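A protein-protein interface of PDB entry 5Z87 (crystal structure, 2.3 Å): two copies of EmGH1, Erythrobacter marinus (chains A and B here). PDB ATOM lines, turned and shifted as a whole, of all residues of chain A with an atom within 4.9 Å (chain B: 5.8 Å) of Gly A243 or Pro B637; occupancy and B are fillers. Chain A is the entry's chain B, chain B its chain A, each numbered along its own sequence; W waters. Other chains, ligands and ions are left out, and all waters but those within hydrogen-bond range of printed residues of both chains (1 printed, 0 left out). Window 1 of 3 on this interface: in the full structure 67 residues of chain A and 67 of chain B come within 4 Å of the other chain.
The side-chain hydroxyl of Tyr B651 is in hydrogen-bond range of the backbone carbonyl oxygen of Gly A243 (2.6 Å). NH1 of Arg A189 is in hydrogen-bond range of O of Leu B636, 2.9 Å away. NH1 of Arg A245 lies within hydrogen-bond range of O of Gln B635. The guanidinium group (NH1) of Arg A245 sits at hydrogen-bond distance from the side-chain hydroxyl (OH) of Tyr B651. The backbone carbonyl oxygen (O) of Gly B634 sits at hydrogen-bond distance from the guanidinium group (NH1) of Arg A189. The guanidinium group (NH2) of Arg A245 lies within hydrogen-bond range of the backbone carbonyl oxygen (O) of Pro B637 (3.0 Å).
No position is printed for both chains. Of the 13 pairs that touch across the chains among the printed residues, none has its exchanged pair printed and touching as well.
Hydrophobic or aromatic side chains of chain B within 4 Å of the printed part of chain A: Pro B637 and Tyr B651. Hydrophobic or aromatic side chains of chain A within 4 Å of the printed part of chain B: Ile A242. Among the printed residues, 13 pairs touch across the chains. Among the printed residues, no Asp or Glu carboxylate lies within 4 Å of a Lys or Arg side-chain nitrogen of the other chain.
The backbone carbonyl oxygen of Tyr B639 lies within hydrogen-bond range of the side-chain amide nitrogen of Gln B642 (2.7 Å). The side-chain carboxylate (OD2) of Asp A187 is in salt-bridge range of the guanidinium group (NH2) of Arg A189.
Of chain B, only Leu B636 (3.2 Å), Pro B637 (3.6 Å) and Tyr B651 (2.6 Å) come within 4 Å of Gly A243. Printed residues of chain B within 4 Å of Arg A245: Gln B635, Pro B637, Gln B642, Arg B647 and Tyr B651. Of the printed residues of chain A, Gln B642 touches Ile A242 and Arg A245. Of the printed residues of chain B, Arg A189 touches Gly B634, Leu B636 and Tyr B651. Of the printed residues of chain B, Ile A242 touches Pro B637 and Gln B642. Gly A241 touches none of the printed residues of chain B. The nearest printed residue of chain A that does not touch Tyr B651 is Gly A244 (4.7 Å).
Water W1 lies within hydrogen-bond range of the backbone carbonyl oxygen of Gln B635 (2.7 Å), the backbone carbonyl oxygen of Pro B637 (3.2 Å), the guanidinium group of Arg A245 (3.4 Å) and the guanidinium group of Arg B647 (3.4 Å).
Among the printed residues, merely in contact across the chains: Gly A243 with Leu B636, Gly A243 with Pro B637, Arg A245 with Gln B642, Arg A245 with Arg B647, Ile A242 with Pro B637, Ile A242 with Gln B642 and Arg A189 with Tyr B651.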
ATOM      1  N   ASP A 187     -24.867  -2.552   9.922  1.00  0.00           N
ATOM      2  CA  ASP A 187     -24.505  -2.732  11.325  1.00  0.00           C
ATOM      3  C   ASP A 187     -23.126  -2.128  11.537  1.00  0.00           C
ATOM      4  O   ASP A 187     -22.103  -2.763  11.225  1.00  0.00           O
ATOM      5  CB  ASP A 187     -24.533  -4.204  11.725  1.00  0.00           C
ATOM      6  CG  ASP A 187     -24.593  -4.405  13.233  1.00  0.00           C
ATOM      7  OD1 ASP A 187     -23.950  -3.638  13.987  1.00  0.00           O
ATOM      8  OD2 ASP A 187     -25.279  -5.354  13.667  1.00  0.00           O
ATOM      9  N   ARG A 189     -21.402  -1.903  14.095  1.00  0.00           N
ATOM     10  CA  ARG A 189     -20.539  -2.659  14.997  1.00  0.00           C
ATOM     11  C   ARG A 189     -19.473  -3.418  14.229  1.00  0.00           C
ATOM     12  O   ARG A 189     -18.409  -3.721  14.779  1.00  0.00           O
ATOM     13  CB  ARG A 189     -21.363  -3.644  15.819  1.00  0.00           C
ATOM     14  CG  ARG A 189     -22.321  -2.983  16.814  1.00  0.00           C
ATOM     15  CD  ARG A 189     -23.110  -4.058  17.558  1.00  0.00           C
ATOM     16  NE  ARG A 189     -24.144  -4.627  16.707  1.00  0.00           N
ATOM     17  CZ  ARG A 189     -25.009  -5.551  17.112  1.00  0.00           C
ATOM     18  NH1 ARG A 189     -24.942  -6.023  18.354  1.00  0.00           N
ATOM     19  NH2 ARG A 189     -25.921  -6.018  16.267  1.00  0.00           N
ATOM     20  N   GLY A 241     -24.037  -9.795   9.007  1.00  0.00           N
ATOM     21  CA  GLY A 241     -23.754 -10.701  10.103  1.00  0.00           C
ATOM     22  C   GLY A 241     -24.351 -10.223  11.420  1.00  0.00           C
ATOM     23  O   GLY A 241     -24.215  -9.048  11.791  1.00  0.00           O
ATOM     24  N   ILE A 242     -25.041 -11.122  12.126  1.00  0.00           N
ATOM     25  CA  ILE A 242     -25.658 -10.747  13.391  1.00  0.00           C
ATOM     26  C   ILE A 242     -24.601 -10.296  14.397  1.00  0.00           C
ATOM     27  O   ILE A 242     -23.435 -10.723  14.361  1.00  0.00           O
ATOM     28  CB  ILE A 242     -26.476 -11.912  13.964  1.00  0.00           C
ATOM     29  CG1 ILE A 242     -25.593 -13.153  14.136  1.00  0.00           C
ATOM     30  CG2 ILE A 242     -27.652 -12.224  13.069  1.00  0.00           C
ATOM     31  CD1 ILE A 242     -26.265 -14.256  14.989  1.00  0.00           C
ATOM     32  N   GLY A 243     -25.025  -9.430  15.313  1.00  0.00           N
ATOM     33  CA  GLY A 243     -24.155  -8.914  16.327  1.00  0.00           C
ATOM     34  C   GLY A 243     -23.065  -8.012  15.818  1.00  0.00           C
ATOM     35  O   GLY A 243     -22.238  -7.566  16.621  1.00  0.00           O
ATOM     36  N   GLY A 244     -23.046  -7.720  14.518  1.00  0.00           N
ATOM     37  CA  GLY A 244     -21.903  -7.094  13.900  1.00  0.00           C
ATOM     38  C   GLY A 244     -20.628  -7.902  14.009  1.00  0.00           C
ATOM     39  O   GLY A 244     -19.533  -7.341  13.886  1.00  0.00           O
ATOM     40  N   ARG A 245     -20.738  -9.206  14.255  1.00  0.00           N
ATOM     41  CA  ARG A 245     -19.573 -10.047  14.477  1.00  0.00           C
ATOM     42  C   ARG A 245     -19.115 -10.641  13.151  1.00  0.00           C
ATOM     43  O   ARG A 245     -19.896 -11.304  12.455  1.00  0.00           O
ATOM     44  CB  ARG A 245     -19.895 -11.147  15.486  1.00  0.00           C
ATOM     45  CG  ARG A 245     -20.479 -10.587  16.779  1.00  0.00           C
ATOM     46  CD  ARG A 245     -20.634 -11.647  17.836  1.00  0.00           C
ATOM     47  NE  ARG A 245     -21.795 -12.496  17.600  1.00  0.00           N
ATOM     48  CZ  ARG A 245     -22.978 -12.341  18.192  1.00  0.00           C
ATOM     49  NH1 ARG A 245     -23.164 -11.368  19.065  1.00  0.00           N
ATOM     50  NH2 ARG A 245     -23.967 -13.184  17.926  1.00  0.00           N
ATOM     51  N   THR B 186     -35.572 -13.945  21.614  1.00  0.00           N
ATOM     52  CA  THR B 186     -34.194 -13.810  21.157  1.00  0.00           C
ATOM     53  C   THR B 186     -33.645 -12.400  21.347  1.00  0.00           C
ATOM     54  O   THR B 186     -32.449 -12.178  21.134  1.00  0.00           O
ATOM     55  CB  THR B 186     -34.074 -14.185  19.671  1.00  0.00           C
ATOM     56  OG1 THR B 186     -34.920 -13.320  18.900  1.00  0.00           O
ATOM     57  CG2 THR B 186     -34.469 -15.639  19.438  1.00  0.00           C
ATOM     58  N   VAL B 630     -26.772 -11.547  28.307  1.00  0.00           N
ATOM     59  CA  VAL B 630     -25.558 -10.976  27.729  1.00  0.00           C
ATOM     60  C   VAL B 630     -25.040  -9.877  28.646  1.00  0.00           C
ATOM     61  O   VAL B 630     -25.771  -9.331  29.473  1.00  0.00           O
ATOM     62  CB  VAL B 630     -25.795 -10.443  26.305  1.00  0.00           C
ATOM     63  CG1 VAL B 630     -26.270 -11.574  25.376  1.00  0.00           C
ATOM     64  CG2 VAL B 630     -26.809  -9.306  26.328  1.00  0.00           C
ATOM     65  N   GLY B 634     -24.989  -4.244  23.376  1.00  0.00           N
ATOM     66  CA  GLY B 634     -24.225  -4.207  22.139  1.00  0.00           C
ATOM     67  C   GLY B 634     -23.733  -5.556  21.656  1.00  0.00           C
ATOM     68  O   GLY B 634     -23.231  -5.659  20.534  1.00  0.00           O
ATOM     69  N   GLN B 635     -23.885  -6.596  22.467  1.00  0.00           N
ATOM     70  CA  GLN B 635     -23.495  -7.951  22.101  1.00  0.00           C
ATOM     71  C   GLN B 635     -24.675  -8.803  21.627  1.00  0.00           C
ATOM     72  O   GLN B 635     -24.507 -10.011  21.423  1.00  0.00           O
ATOM     73  CB  GLN B 635     -22.793  -8.621  23.292  1.00  0.00           C
ATOM     74  CG  GLN B 635     -21.766  -7.706  23.966  1.00  0.00           C
ATOM     75  CD  GLN B 635     -20.803  -8.434  24.870  1.00  0.00           C
ATOM     76  OE1 GLN B 635     -21.068  -9.547  25.315  1.00  0.00           O
ATOM     77  NE2 GLN B 635     -19.658  -7.823  25.123  1.00  0.00           N
ATOM     78  N   LEU B 636     -25.860  -8.212  21.452  1.00  0.00           N
ATOM     79  CA  LEU B 636     -27.001  -8.988  20.979  1.00  0.00           C
ATOM     80  C   LEU B 636     -26.816  -9.358  19.502  1.00  0.00           C
ATOM     81  O   LEU B 636     -26.302  -8.556  18.713  1.00  0.00           O
ATOM     82  CB  LEU B 636     -28.294  -8.200  21.169  1.00  0.00           C
ATOM     83  CG  LEU B 636     -28.731  -7.964  22.615  1.00  0.00           C
ATOM     84  CD1 LEU B 636     -29.986  -7.119  22.666  1.00  0.00           C
ATOM     85  CD2 LEU B 636     -28.965  -9.283  23.325  1.00  0.00           C
ATOM     86  N   PRO B 637     -27.231 -10.559  19.087  1.00  0.00           N
ATOM     87  CA  PRO B 637     -27.893 -11.577  19.913  1.00  0.00           C
ATOM     88  C   PRO B 637     -26.922 -12.443  20.665  1.00  0.00           C
ATOM     89  O   PRO B 637     -25.792 -12.628  20.185  1.00  0.00           O
ATOM     90  CB  PRO B 637     -28.668 -12.420  18.887  1.00  0.00           C
ATOM     91  CG  PRO B 637     -27.917 -12.282  17.653  1.00  0.00           C
ATOM     92  CD  PRO B 637     -27.268 -10.906  17.656  1.00  0.00           C
ATOM     93  N   GLY B 638     -27.374 -12.991  21.800  1.00  0.00           N
ATOM     94  CA  GLY B 638     -26.551 -13.880  22.586  1.00  0.00           C
ATOM     95  C   GLY B 638     -27.156 -15.224  22.943  1.00  0.00           C
ATOM     96  O   GLY B 638     -26.571 -15.954  23.746  1.00  0.00           O
ATOM     97  N   TYR B 639     -28.295 -15.581  22.352  1.00  0.00           N
ATOM     98  CA  TYR B 639     -28.916 -16.854  22.684  1.00  0.00           C
ATOM     99  C   TYR B 639     -27.942 -17.998  22.410  1.00  0.00           C
ATOM    100  O   TYR B 639     -27.156 -17.962  21.456  1.00  0.00           O
ATOM    101  CB  TYR B 639     -30.229 -17.038  21.905  1.00  0.00           C
ATOM    102  CG  TYR B 639     -30.102 -16.904  20.397  1.00  0.00           C
ATOM    103  CD1 TYR B 639     -29.674 -17.977  19.618  1.00  0.00           C
ATOM    104  CD2 TYR B 639     -30.426 -15.708  19.756  1.00  0.00           C
ATOM    105  CE1 TYR B 639     -29.554 -17.862  18.241  1.00  0.00           C
ATOM    106  CE2 TYR B 639     -30.317 -15.578  18.386  1.00  0.00           C
ATOM    107  CZ  TYR B 639     -29.877 -16.659  17.623  1.00  0.00           C
ATOM    108  OH  TYR B 639     -29.749 -16.538  16.243  1.00  0.00           O
ATOM    109  N   GLN B 642     -26.154 -20.777  19.106  1.00  0.00           N
ATOM    110  CA  GLN B 642     -25.550 -20.125  17.955  1.00  0.00           C
ATOM    111  C   GLN B 642     -25.142 -21.165  16.919  1.00  0.00           C
ATOM    112  O   GLN B 642     -24.847 -22.315  17.244  1.00  0.00           O
ATOM    113  CB  GLN B 642     -24.320 -19.311  18.376  1.00  0.00           C
ATOM    114  CG  GLN B 642     -24.608 -18.166  19.349  1.00  0.00           C
ATOM    115  CD  GLN B 642     -25.350 -17.031  18.681  1.00  0.00           C
ATOM    116  OE1 GLN B 642     -24.987 -16.600  17.589  1.00  0.00           O
ATOM    117  NE2 GLN B 642     -26.420 -16.556  19.320  1.00  0.00           N
ATOM    118  N   ARG B 647     -21.091 -16.777  17.234  1.00  0.00           N
ATOM    119  CA  ARG B 647     -20.210 -16.061  18.143  1.00  0.00           C
ATOM    120  C   ARG B 647     -18.776 -16.525  17.938  1.00  0.00           C
ATOM    121  O   ARG B 647     -18.004 -16.652  18.878  1.00  0.00           O
ATOM    122  CB  ARG B 647     -20.671 -16.221  19.595  1.00  0.00           C
ATOM    123  CG  ARG B 647     -21.942 -15.389  19.898  1.00  0.00           C
ATOM    124  CD  ARG B 647     -22.495 -15.631  21.296  1.00  0.00           C
ATOM    125  NE  ARG B 647     -21.560 -15.204  22.336  1.00  0.00           N
ATOM    126  CZ  ARG B 647     -20.821 -16.045  23.048  1.00  0.00           C
ATOM    127  NH1 ARG B 647     -20.910 -17.358  22.826  1.00  0.00           N
ATOM    128  NH2 ARG B 647     -20.004 -15.585  23.987  1.00  0.00           N
ATOM    129  N   TYR B 651     -15.752  -9.371  20.716  1.00  0.00           N
ATOM    130  CA  TYR B 651     -15.743  -7.917  20.607  1.00  0.00           C
ATOM    131  C   TYR B 651     -14.423  -7.359  21.123  1.00  0.00           C
ATOM    132  O   TYR B 651     -13.873  -7.842  22.116  1.00  0.00           O
ATOM    133  CB  TYR B 651     -16.920  -7.315  21.380  1.00  0.00           C
ATOM    134  CG  TYR B 651     -18.263  -7.642  20.761  1.00  0.00           C
ATOM    135  CD1 TYR B 651     -18.695  -6.987  19.617  1.00  0.00           C
ATOM    136  CD2 TYR B 651     -19.086  -8.623  21.310  1.00  0.00           C
ATOM    137  CE1 TYR B 651     -19.917  -7.277  19.044  1.00  0.00           C
ATOM    138  CE2 TYR B 651     -20.304  -8.927  20.750  1.00  0.00           C
ATOM    139  CZ  TYR B 651     -20.719  -8.258  19.610  1.00  0.00           C
ATOM    140  OH  TYR B 651     -21.937  -8.569  19.040  1.00  0.00           O
HETATM  141  O   HOH W   1     -23.373 -12.306  22.314  1.00  0.00           O
